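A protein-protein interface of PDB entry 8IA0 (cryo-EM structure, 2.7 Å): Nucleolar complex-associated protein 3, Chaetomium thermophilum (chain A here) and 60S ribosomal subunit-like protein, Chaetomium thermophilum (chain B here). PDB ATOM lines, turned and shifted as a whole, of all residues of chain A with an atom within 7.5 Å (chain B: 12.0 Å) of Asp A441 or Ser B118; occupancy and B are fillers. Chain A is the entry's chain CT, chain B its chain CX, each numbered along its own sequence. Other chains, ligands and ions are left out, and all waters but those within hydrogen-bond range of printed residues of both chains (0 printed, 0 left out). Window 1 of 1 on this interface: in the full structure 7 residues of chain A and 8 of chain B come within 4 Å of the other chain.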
ATOM      1  N   PHE A 409       5.645   7.242 -35.790  1.00  0.00           N
ATOM      2  CA  PHE A 409       4.785   6.272 -35.123  1.00  0.00           C
ATOM      3  C   PHE A 409       3.392   6.240 -35.737  1.00  0.00           C
ATOM      4  O   PHE A 409       2.764   5.178 -35.803  1.00  0.00           O
ATOM      5  CB  PHE A 409       4.710   6.580 -33.632  1.00  0.00           C
ATOM      6  CG  PHE A 409       5.997   6.343 -32.902  1.00  0.00           C
ATOM      7  CD1 PHE A 409       6.943   5.476 -33.411  1.00  0.00           C
ATOM      8  CD2 PHE A 409       6.260   6.985 -31.708  1.00  0.00           C
ATOM      9  CE1 PHE A 409       8.124   5.256 -32.744  1.00  0.00           C
ATOM     10  CE2 PHE A 409       7.438   6.765 -31.038  1.00  0.00           C
ATOM     11  CZ  PHE A 409       8.373   5.903 -31.557  1.00  0.00           C
ATOM     12  N   ASN A 435      15.154   9.534 -24.868  1.00  0.00           N
ATOM     13  CA  ASN A 435      15.283   9.066 -23.497  1.00  0.00           C
ATOM     14  C   ASN A 435      15.475   7.550 -23.458  1.00  0.00           C
ATOM     15  O   ASN A 435      15.035   6.812 -24.344  1.00  0.00           O
ATOM     16  CB  ASN A 435      14.064   9.491 -22.686  1.00  0.00           C
ATOM     17  CG  ASN A 435      14.008  10.988 -22.468  1.00  0.00           C
ATOM     18  OD1 ASN A 435      15.039  11.654 -22.400  1.00  0.00           O
ATOM     19  ND2 ASN A 435      12.801  11.527 -22.363  1.00  0.00           N
ATOM     20  N   GLN A 436      16.158   7.085 -22.408  1.00  0.00           N
ATOM     21  CA  GLN A 436      16.490   5.669 -22.277  1.00  0.00           C
ATOM     22  C   GLN A 436      15.244   4.798 -22.192  1.00  0.00           C
ATOM     23  O   GLN A 436      15.149   3.764 -22.861  1.00  0.00           O
ATOM     24  CB  GLN A 436      17.359   5.441 -21.039  1.00  0.00           C
ATOM     25  CG  GLN A 436      18.797   5.859 -21.175  1.00  0.00           C
ATOM     26  CD  GLN A 436      19.615   5.456 -19.970  1.00  0.00           C
ATOM     27  OE1 GLN A 436      20.842   5.534 -19.982  1.00  0.00           O
ATOM     28  NE2 GLN A 436      18.938   5.012 -18.920  1.00  0.00           N
ATOM     29  N   ASP A 437      14.285   5.197 -21.356  1.00  0.00           N
ATOM     30  CA  ASP A 437      13.111   4.363 -21.122  1.00  0.00           C
ATOM     31  C   ASP A 437      12.288   4.184 -22.392  1.00  0.00           C
ATOM     32  O   ASP A 437      11.503   3.234 -22.502  1.00  0.00           O
ATOM     33  CB  ASP A 437      12.266   4.965 -20.002  1.00  0.00           C
ATOM     34  CG  ASP A 437      12.193   6.473 -20.075  1.00  0.00           C
ATOM     35  OD1 ASP A 437      13.170   7.135 -19.667  1.00  0.00           O
ATOM     36  OD2 ASP A 437      11.160   6.999 -20.540  1.00  0.00           O
ATOM     37  N   PHE A 438      12.450   5.083 -23.364  1.00  0.00           N
ATOM     38  CA  PHE A 438      11.745   4.920 -24.630  1.00  0.00           C
ATOM     39  C   PHE A 438      12.471   3.960 -25.564  1.00  0.00           C
ATOM     40  O   PHE A 438      11.879   3.489 -26.540  1.00  0.00           O
ATOM     41  CB  PHE A 438      11.555   6.274 -25.314  1.00  0.00           C
ATOM     42  CG  PHE A 438      10.562   7.175 -24.632  1.00  0.00           C
ATOM     43  CD1 PHE A 438       9.955   6.800 -23.447  1.00  0.00           C
ATOM     44  CD2 PHE A 438      10.243   8.404 -25.177  1.00  0.00           C
ATOM     45  CE1 PHE A 438       9.050   7.631 -22.823  1.00  0.00           C
ATOM     46  CE2 PHE A 438       9.337   9.238 -24.556  1.00  0.00           C
ATOM     47  CZ  PHE A 438       8.741   8.850 -23.378  1.00  0.00           C
ATOM     48  N   PHE A 439      13.744   3.660 -25.293  1.00  0.00           N
ATOM     49  CA  PHE A 439      14.480   2.754 -26.169  1.00  0.00           C
ATOM     50  C   PHE A 439      13.954   1.329 -26.053  1.00  0.00           C
ATOM     51  O   PHE A 439      13.806   0.632 -27.062  1.00  0.00           O
ATOM     52  CB  PHE A 439      15.976   2.813 -25.856  1.00  0.00           C
ATOM     53  CG  PHE A 439      16.856   2.323 -26.976  1.00  0.00           C
ATOM     54  CD1 PHE A 439      16.822   1.002 -27.387  1.00  0.00           C
ATOM     55  CD2 PHE A 439      17.711   3.192 -27.626  1.00  0.00           C
ATOM     56  CE1 PHE A 439      17.625   0.559 -28.415  1.00  0.00           C
ATOM     57  CE2 PHE A 439      18.517   2.753 -28.656  1.00  0.00           C
ATOM     58  CZ  PHE A 439      18.473   1.436 -29.050  1.00  0.00           C
ATOM     59  N   GLY A 440      13.664   0.880 -24.832  1.00  0.00           N
ATOM     60  CA  GLY A 440      13.055  -0.428 -24.666  1.00  0.00           C
ATOM     61  C   GLY A 440      11.665  -0.501 -25.267  1.00  0.00           C
ATOM     62  O   GLY A 440      11.226  -1.562 -25.717  1.00  0.00           O
ATOM     63  N   ASP A 441      10.950   0.625 -25.275  1.00  0.00           N
ATOM     64  CA  ASP A 441       9.620   0.656 -25.875  1.00  0.00           C
ATOM     65  C   ASP A 441       9.689   0.457 -27.383  1.00  0.00           C
ATOM     66  O   ASP A 441       8.788  -0.145 -27.978  1.00  0.00           O
ATOM     67  CB  ASP A 441       8.925   1.974 -25.543  1.00  0.00           C
ATOM     68  CG  ASP A 441       8.894   2.257 -24.058  1.00  0.00           C
ATOM     69  OD1 ASP A 441       9.270   1.361 -23.275  1.00  0.00           O
ATOM     70  OD2 ASP A 441       8.494   3.376 -23.672  1.00  0.00           O
ATOM     71  N   LEU A 442      10.743   0.969 -28.021  1.00  0.00           N
ATOM     72  CA  LEU A 442      10.881   0.808 -29.464  1.00  0.00           C
ATOM     73  C   LEU A 442      11.008  -0.660 -29.845  1.00  0.00           C
ATOM     74  O   LEU A 442      10.416  -1.105 -30.835  1.00  0.00           O
ATOM     75  CB  LEU A 442      12.086   1.598 -29.970  1.00  0.00           C
ATOM     76  CG  LEU A 442      12.017   3.114 -29.799  1.00  0.00           C
ATOM     77  CD1 LEU A 442      13.323   3.759 -30.221  1.00  0.00           C
ATOM     78  CD2 LEU A 442      10.861   3.680 -30.594  1.00  0.00           C
ATOM     79  N   LEU A 443      11.779  -1.429 -29.074  1.00  0.00           N
ATOM     80  CA  LEU A 443      11.878  -2.862 -29.333  1.00  0.00           C
ATOM     81  C   LEU A 443      10.533  -3.547 -29.138  1.00  0.00           C
ATOM     82  O   LEU A 443      10.148  -4.412 -29.934  1.00  0.00           O
ATOM     83  CB  LEU A 443      12.936  -3.491 -28.430  1.00  0.00           C
ATOM     84  CG  LEU A 443      14.392  -3.283 -28.840  1.00  0.00           C
ATOM     85  CD1 LEU A 443      15.326  -3.992 -27.875  1.00  0.00           C
ATOM     86  CD2 LEU A 443      14.620  -3.763 -30.261  1.00  0.00           C
ATOM     87  N   GLU A 444       9.807  -3.178 -28.083  1.00  0.00           N
ATOM     88  CA  GLU A 444       8.500  -3.775 -27.841  1.00  0.00           C
ATOM     89  C   GLU A 444       7.520  -3.421 -28.953  1.00  0.00           C
ATOM     90  O   GLU A 444       6.701  -4.254 -29.357  1.00  0.00           O
ATOM     91  CB  GLU A 444       7.965  -3.324 -26.485  1.00  0.00           C
ATOM     92  CG  GLU A 444       7.239  -4.406 -25.714  1.00  0.00           C
ATOM     93  CD  GLU A 444       8.139  -5.572 -25.364  1.00  0.00           C
ATOM     94  OE1 GLU A 444       7.645  -6.718 -25.331  1.00  0.00           O
ATOM     95  OE2 GLU A 444       9.341  -5.343 -25.119  1.00  0.00           O
ATOM     96  N   ALA A 445       7.585  -2.187 -29.454  1.00  0.00           N
ATOM     97  CA  ALA A 445       6.735  -1.796 -30.575  1.00  0.00           C
ATOM     98  C   ALA A 445       7.080  -2.587 -31.830  1.00  0.00           C
ATOM     99  O   ALA A 445       6.191  -2.933 -32.617  1.00  0.00           O
ATOM    100  CB  ALA A 445       6.861  -0.296 -30.833  1.00  0.00           C
ATOM    101  N   LEU A 446       8.367  -2.872 -32.041  1.00  0.00           N
ATOM    102  CA  LEU A 446       8.769  -3.693 -33.177  1.00  0.00           C
ATOM    103  C   LEU A 446       8.197  -5.100 -33.072  1.00  0.00           C
ATOM    104  O   LEU A 446       7.771  -5.682 -34.076  1.00  0.00           O
ATOM    105  CB  LEU A 446      10.292  -3.743 -33.277  1.00  0.00           C
ATOM    106  CG  LEU A 446      11.010  -2.464 -33.706  1.00  0.00           C
ATOM    107  CD1 LEU A 446      12.507  -2.632 -33.555  1.00  0.00           C
ATOM    108  CD2 LEU A 446      10.655  -2.103 -35.134  1.00  0.00           C
ATOM    109  N   LYS A 447       8.190  -5.667 -31.863  1.00  0.00           N
ATOM    110  CA  LYS A 447       7.677  -7.019 -31.679  1.00  0.00           C
ATOM    111  C   LYS A 447       6.196  -7.100 -32.026  1.00  0.00           C
ATOM    112  O   LYS A 447       5.740  -8.091 -32.607  1.00  0.00           O
ATOM    113  CB  LYS A 447       7.916  -7.479 -30.243  1.00  0.00           C
ATOM    114  CG  LYS A 447       9.382  -7.569 -29.853  1.00  0.00           C
ATOM    115  CD  LYS A 447       9.569  -8.405 -28.598  1.00  0.00           C
ATOM    116  CE  LYS A 447      10.882  -8.083 -27.907  1.00  0.00           C
ATOM    117  NZ  LYS A 447      10.698  -7.843 -26.452  1.00  0.00           N
ATOM    118  N   LEU A 505      19.524  -1.774 -19.713  1.00  0.00           N
ATOM    119  CA  LEU A 505      18.207  -1.464 -20.255  1.00  0.00           C
ATOM    120  C   LEU A 505      17.413  -2.695 -20.672  1.00  0.00           C
ATOM    121  O   LEU A 505      16.308  -2.544 -21.202  1.00  0.00           O
ATOM    122  CB  LEU A 505      18.330  -0.503 -21.443  1.00  0.00           C
ATOM    123  CG  LEU A 505      18.593   0.993 -21.221  1.00  0.00           C
ATOM    124  CD1 LEU A 505      19.757   1.284 -20.289  1.00  0.00           C
ATOM    125  CD2 LEU A 505      18.798   1.684 -22.560  1.00  0.00           C
ATOM    126  N   HIS A 506      17.938  -3.900 -20.446  1.00  0.00           N
ATOM    127  CA  HIS A 506      17.227  -5.149 -20.721  1.00  0.00           C
ATOM    128  C   HIS A 506      16.781  -5.225 -22.182  1.00  0.00           C
ATOM    129  O   HIS A 506      15.596  -5.337 -22.495  1.00  0.00           O
ATOM    130  CB  HIS A 506      16.028  -5.314 -19.779  1.00  0.00           C
ATOM    131  CG  HIS A 506      16.400  -5.426 -18.335  1.00  0.00           C
ATOM    132  ND1 HIS A 506      16.384  -4.348 -17.477  1.00  0.00           N
ATOM    133  CD2 HIS A 506      16.784  -6.491 -17.595  1.00  0.00           C
ATOM    134  CE1 HIS A 506      16.750  -4.743 -16.272  1.00  0.00           C
ATOM    135  NE2 HIS A 506      16.999  -6.039 -16.316  1.00  0.00           N
ATOM    136  N   LEU A 507      17.757  -5.156 -23.079  1.00  0.00           N
ATOM    137  CA  LEU A 507      17.509  -5.234 -24.515  1.00  0.00           C
ATOM    138  C   LEU A 507      17.926  -6.621 -24.990  1.00  0.00           C
ATOM    139  O   LEU A 507      19.098  -6.855 -25.301  1.00  0.00           O
ATOM    140  CB  LEU A 507      18.255  -4.133 -25.261  1.00  0.00           C
ATOM    141  CG  LEU A 507      18.152  -2.727 -24.668  1.00  0.00           C
ATOM    142  CD1 LEU A 507      19.232  -1.823 -25.232  1.00  0.00           C
ATOM    143  CD2 LEU A 507      16.778  -2.139 -24.920  1.00  0.00           C
ATOM    144  N   ALA B 110       9.716 -12.942 -13.167  1.00  0.00           N
ATOM    145  CA  ALA B 110       9.482 -11.523 -12.923  1.00  0.00           C
ATOM    146  C   ALA B 110      10.263 -11.033 -11.711  1.00  0.00           C
ATOM    147  O   ALA B 110      10.839  -9.939 -11.736  1.00  0.00           O
ATOM    148  CB  ALA B 110       7.988 -11.263 -12.738  1.00  0.00           C
ATOM    149  N   GLN B 113      14.074 -10.727 -12.569  1.00  0.00           N
ATOM    150  CA  GLN B 113      14.383  -9.604 -13.449  1.00  0.00           C
ATOM    151  C   GLN B 113      14.405  -8.293 -12.672  1.00  0.00           C
ATOM    152  O   GLN B 113      15.286  -7.451 -12.876  1.00  0.00           O
ATOM    153  CB  GLN B 113      13.370  -9.541 -14.589  1.00  0.00           C
ATOM    154  CG  GLN B 113      13.736  -8.567 -15.687  1.00  0.00           C
ATOM    155  CD  GLN B 113      13.500  -9.141 -17.068  1.00  0.00           C
ATOM    156  OE1 GLN B 113      14.413  -9.205 -17.891  1.00  0.00           O
ATOM    157  NE2 GLN B 113      12.271  -9.565 -17.329  1.00  0.00           N
ATOM    158  N   GLY B 114      13.440  -8.105 -11.779  1.00  0.00           N
ATOM    159  CA  GLY B 114      13.438  -6.953 -10.901  1.00  0.00           C
ATOM    160  C   GLY B 114      12.970  -5.664 -11.539  1.00  0.00           C
ATOM    161  O   GLY B 114      11.823  -5.561 -11.984  1.00  0.00           O
ATOM    162  N   GLN B 115      13.855  -4.673 -11.594  1.00  0.00           N
ATOM    163  CA  GLN B 115      13.492  -3.326 -12.012  1.00  0.00           C
ATOM    164  C   GLN B 115      13.741  -3.160 -13.506  1.00  0.00           C
ATOM    165  O   GLN B 115      14.851  -3.409 -13.988  1.00  0.00           O
ATOM    166  CB  GLN B 115      14.284  -2.289 -11.219  1.00  0.00           C
ATOM    167  CG  GLN B 115      13.855  -0.858 -11.472  1.00  0.00           C
ATOM    168  CD  GLN B 115      12.596  -0.488 -10.717  1.00  0.00           C
ATOM    169  OE1 GLN B 115      11.486  -0.654 -11.221  1.00  0.00           O
ATOM    170  NE2 GLN B 115      12.763   0.017  -9.502  1.00  0.00           N
ATOM    171  N   ILE B 116      12.709  -2.738 -14.232  1.00  0.00           N
ATOM    172  CA  ILE B 116      12.800  -2.447 -15.658  1.00  0.00           C
ATOM    173  C   ILE B 116      12.448  -0.981 -15.862  1.00  0.00           C
ATOM    174  O   ILE B 116      11.406  -0.516 -15.387  1.00  0.00           O
ATOM    175  CB  ILE B 116      11.876  -3.353 -16.490  1.00  0.00           C
ATOM    176  CG1 ILE B 116      12.066  -4.819 -16.093  1.00  0.00           C
ATOM    177  CG2 ILE B 116      12.132  -3.145 -17.971  1.00  0.00           C
ATOM    178  CD1 ILE B 116      11.649  -5.806 -17.163  1.00  0.00           C
ATOM    179  N   GLU B 117      13.316  -0.257 -16.570  1.00  0.00           N
ATOM    180  CA  GLU B 117      13.128   1.174 -16.767  1.00  0.00           C
ATOM    181  C   GLU B 117      12.020   1.499 -17.759  1.00  0.00           C
ATOM    182  O   GLU B 117      11.380   2.547 -17.628  1.00  0.00           O
ATOM    183  CB  GLU B 117      14.436   1.815 -17.234  1.00  0.00           C
ATOM    184  CG  GLU B 117      14.856   3.021 -16.416  1.00  0.00           C
ATOM    185  CD  GLU B 117      16.166   3.617 -16.886  1.00  0.00           C
ATOM    186  OE1 GLU B 117      16.673   3.183 -17.942  1.00  0.00           O
ATOM    187  OE2 GLU B 117      16.690   4.519 -16.200  1.00  0.00           O
ATOM    188  N   SER B 118      11.780   0.637 -18.741  1.00  0.00           N
ATOM    189  CA  SER B 118      10.764   0.880 -19.757  1.00  0.00           C
ATOM    190  C   SER B 118       9.382   0.614 -19.173  1.00  0.00           C
ATOM    191  O   SER B 118       9.167  -0.412 -18.517  1.00  0.00           O
ATOM    192  CB  SER B 118      11.009  -0.001 -20.979  1.00  0.00           C
ATOM    193  OG  SER B 118      12.245   0.316 -21.594  1.00  0.00           O
ATOM    194  N   LYS B 119       8.449   1.537 -19.412  1.00  0.00           N
ATOM    195  CA  LYS B 119       7.080   1.336 -18.950  1.00  0.00           C
ATOM    196  C   LYS B 119       6.384   0.237 -19.744  1.00  0.00           C
ATOM    197  O   LYS B 119       5.622  -0.557 -19.180  1.00  0.00           O
ATOM    198  CB  LYS B 119       6.293   2.641 -19.044  1.00  0.00           C
ATOM    199  CG  LYS B 119       6.932   3.809 -18.321  1.00  0.00           C
ATOM    200  CD  LYS B 119       5.971   4.982 -18.222  1.00  0.00           C
ATOM    201  CE  LYS B 119       4.951   4.783 -17.111  1.00  0.00           C
ATOM    202  NZ  LYS B 119       5.401   3.793 -16.093  1.00  0.00           N
ATOM    203  N   ILE B 120       6.626   0.180 -21.054  1.00  0.00           N
ATOM    204  CA  ILE B 120       5.987  -0.840 -21.879  1.00  0.00           C
ATOM    205  C   ILE B 120       6.525  -2.223 -21.535  1.00  0.00           C
ATOM    206  O   ILE B 120       5.763  -3.192 -21.441  1.00  0.00           O
ATOM    207  CB  ILE B 120       6.167  -0.514 -23.371  1.00  0.00           C
ATOM    208  CG1 ILE B 120       5.632   0.886 -23.673  1.00  0.00           C
ATOM    209  CG2 ILE B 120       5.467  -1.551 -24.229  1.00  0.00           C
ATOM    210  CD1 ILE B 120       5.389   1.150 -25.144  1.00  0.00           C
ATOM    211  N   MET B 121       7.841  -2.340 -21.346  1.00  0.00           N
ATOM    212  CA  MET B 121       8.419  -3.635 -21.001  1.00  0.00           C
ATOM    213  C   MET B 121       7.943  -4.108 -19.633  1.00  0.00           C
ATOM    214  O   MET B 121       7.775  -5.312 -19.411  1.00  0.00           O
ATOM    215  CB  MET B 121       9.943  -3.562 -21.047  1.00  0.00           C
ATOM    216  CG  MET B 121      10.505  -3.320 -22.435  1.00  0.00           C
ATOM    217  SD  MET B 121      12.306  -3.329 -22.476  1.00  0.00           S
ATOM    218  CE  MET B 121      12.658  -4.591 -21.258  1.00  0.00           C
ATOM    219  N   ARG B 122       7.727  -3.177 -18.701  1.00  0.00           N
ATOM    220  CA  ARG B 122       7.149  -3.546 -17.413  1.00  0.00           C
ATOM    221  C   ARG B 122       5.724  -4.052 -17.578  1.00  0.00           C
ATOM    222  O   ARG B 122       5.319  -5.017 -16.920  1.00  0.00           O
ATOM    223  CB  ARG B 122       7.188  -2.356 -16.457  1.00  0.00           C
ATOM    224  CG  ARG B 122       8.365  -2.369 -15.502  1.00  0.00           C
ATOM    225  CD  ARG B 122       8.153  -1.399 -14.350  1.00  0.00           C
ATOM    226  NE  ARG B 122       7.666  -0.103 -14.803  1.00  0.00           N
ATOM    227  CZ  ARG B 122       8.375   1.016 -14.767  1.00  0.00           C
ATOM    228  NH1 ARG B 122       9.615   1.034 -14.305  1.00  0.00           N
ATOM    229  NH2 ARG B 122       7.829   2.145 -15.208  1.00  0.00           N
ATOM    230  N   ALA B 123       4.945  -3.406 -18.447  1.00  0.00           N
ATOM    231  CA  ALA B 123       3.569  -3.834 -18.674  1.00  0.00           C
ATOM    232  C   ALA B 123       3.514  -5.233 -19.270  1.00  0.00           C
ATOM    233  O   ALA B 123       2.675  -6.051 -18.874  1.00  0.00           O
ATOM    234  CB  ALA B 123       2.854  -2.837 -19.581  1.00  0.00           C
ATOM    235  N   ARG B 124       4.395  -5.526 -20.229  1.00  0.00           N
ATOM    236  CA  ARG B 124       4.372  -6.830 -20.882  1.00  0.00           C
ATOM    237  C   ARG B 124       4.706  -7.947 -19.903  1.00  0.00           C
ATOM    238  O   ARG B 124       4.119  -9.033 -19.969  1.00  0.00           O
ATOM    239  CB  ARG B 124       5.340  -6.840 -22.063  1.00  0.00           C
ATOM    240  CG  ARG B 124       4.945  -5.896 -23.181  1.00  0.00           C
ATOM    241  CD  ARG B 124       3.803  -6.458 -23.999  1.00  0.00           C
ATOM    242  NE  ARG B 124       3.046  -5.405 -24.662  1.00  0.00           N
ATOM    243  CZ  ARG B 124       3.265  -4.993 -25.902  1.00  0.00           C
ATOM    244  NH1 ARG B 124       4.218  -5.526 -26.650  1.00  0.00           N
ATOM    245  NH2 ARG B 124       2.508  -4.022 -26.407  1.00  0.00           N
ATOM    246  N   GLN B 125       5.648  -7.701 -18.992  1.00  0.00           N
ATOM    247  CA  GLN B 125       5.996  -8.705 -17.993  1.00  0.00           C
ATOM    248  C   GLN B 125       4.811  -9.002 -17.081  1.00  0.00           C
ATOM    249  O   GLN B 125       4.556 -10.160 -16.732  1.00  0.00           O
ATOM    250  CB  GLN B 125       7.204  -8.230 -17.186  1.00  0.00           C
ATOM    251  CG  GLN B 125       7.432  -8.975 -15.890  1.00  0.00           C
ATOM    252  CD  GLN B 125       8.453  -8.291 -15.006  1.00  0.00           C
ATOM    253  OE1 GLN B 125       8.224  -8.090 -13.814  1.00  0.00           O
ATOM    254  NE2 GLN B 125       9.587  -7.926 -15.587  1.00  0.00           N
ATOM    255  N   LEU B 126       4.077  -7.964 -16.680  1.00  0.00           N
ATOM    256  CA  LEU B 126       2.870  -8.178 -15.889  1.00  0.00           C
ATOM    257  C   LEU B 126       1.790  -8.873 -16.709  1.00  0.00           C
ATOM    258  O   LEU B 126       1.040  -9.704 -16.185  1.00  0.00           O
ATOM    259  CB  LEU B 126       2.347  -6.846 -15.350  1.00  0.00           C
ATOM    260  CG  LEU B 126       3.157  -6.143 -14.263  1.00  0.00           C
ATOM    261  CD1 LEU B 126       2.802  -4.669 -14.222  1.00  0.00           C
ATOM    262  CD2 LEU B 126       2.912  -6.789 -12.913  1.00  0.00           C
ATOM    263  N   GLU B 127       1.695  -8.538 -17.997  1.00  0.00           N
ATOM    264  CA  GLU B 127       0.620  -9.071 -18.827  1.00  0.00           C
ATOM    265  C   GLU B 127       0.789 -10.564 -19.077  1.00  0.00           C
ATOM    266  O   GLU B 127      -0.201 -11.302 -19.131  1.00  0.00           O
ATOM    267  CB  GLU B 127       0.556  -8.308 -20.148  1.00  0.00           C
ATOM    268  CG  GLU B 127      -0.646  -8.649 -21.007  1.00  0.00           C
ATOM    269  CD  GLU B 127      -1.120  -7.472 -21.833  1.00  0.00           C
ATOM    270  OE1 GLU B 127      -1.003  -6.325 -21.354  1.00  0.00           O
ATOM    271  OE2 GLU B 127      -1.611  -7.693 -22.961  1.00  0.00           O
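The side-chain hydroxyl (OG) of Ser B118 lies within hydrogen-bond range of the backbone carbonyl oxygen (O) of Asp A437.
NE2 of Gln A436 sits at hydrogen-bond distance from OE1 of Glu B117 (3.1 Å).
NH1 of Arg B124 is in salt-bridge range of OE1 of Glu A444, 3.9 Å away.
NZ of Lys A447 is in salt-bridge range of OE2 of Glu A444 (3.1 Å).
The side-chain hydroxyl (OG) of Ser B118 sits at hydrogen-bond distance from the side-chain sulfur (SD) of Met B121 (3.8 Å).
Hydrophobic or aromatic side chains of chain B within 4 Å of the printed part of chain A: Ile B120 and Met B121.
Among the printed residues, Asp or Glu carboxylates within 4 Å of a Lys or Arg side-chain nitrogen of the other chain: Glu A444 with Arg B124 (3.9 Å).
O of Glu B117 touches CB of Asp A437 (3.5 Å).
Ser B118 touches Gly A440 (OG to CA, 3.3 Å).
Met B121 touches Gly A440.
Asp A441 touches Ser B118 (OD1 to CB, 3.2 Å).
N of Lys B119 touches OD1 of Asp A441 (3.95 Å).
Ile B120 touches Glu A444.
OE2 of Glu A444 touches CG of Met B121 (3.6 Å).
His A506 touches Gln B113 (CD2 to OE1, 3.6 Å).
CE1 of His A506 touches O of Gln B115, 3.3 Å away.
CE of Met B121 touches O of His A506 (3.3 Å).
No residue of chain B comes within 4 Å of Phe A438.
Asp A441 touches just these residues of chain B: Ser B118 (3.2 Å), Lys B119 (3.95 Å) and Ile B120 (3.6 Å).
Glu A444 touches just these residues of chain B: Ile B120, Met B121 and Arg B124.
Ala A445 touches none of the printed residues of chain B.
Of the printed residues of chain A, Gln B113 touches His A506 (3.6 Å).
Of chain A, only Asp A437, Gly A440 and Asp A441 come within 4 Å of Ser B118.
Printed residues of chain A within 4 Å of Ile B120: Asp A441 and Glu A444.
Printed residues of chain A within 4 Å of Arg B124: Glu A444 (3.4 Å).
The nearest residue of chain B that does not touch Asp A441 is Met B121 (4.4 Å).
The nearest residue of chain A that does not touch Ser B118 is Gln A436 (4.7 Å).
The nearest printed residue of chain B that does not touch His A506 is Ile B116 (4.4 Å).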
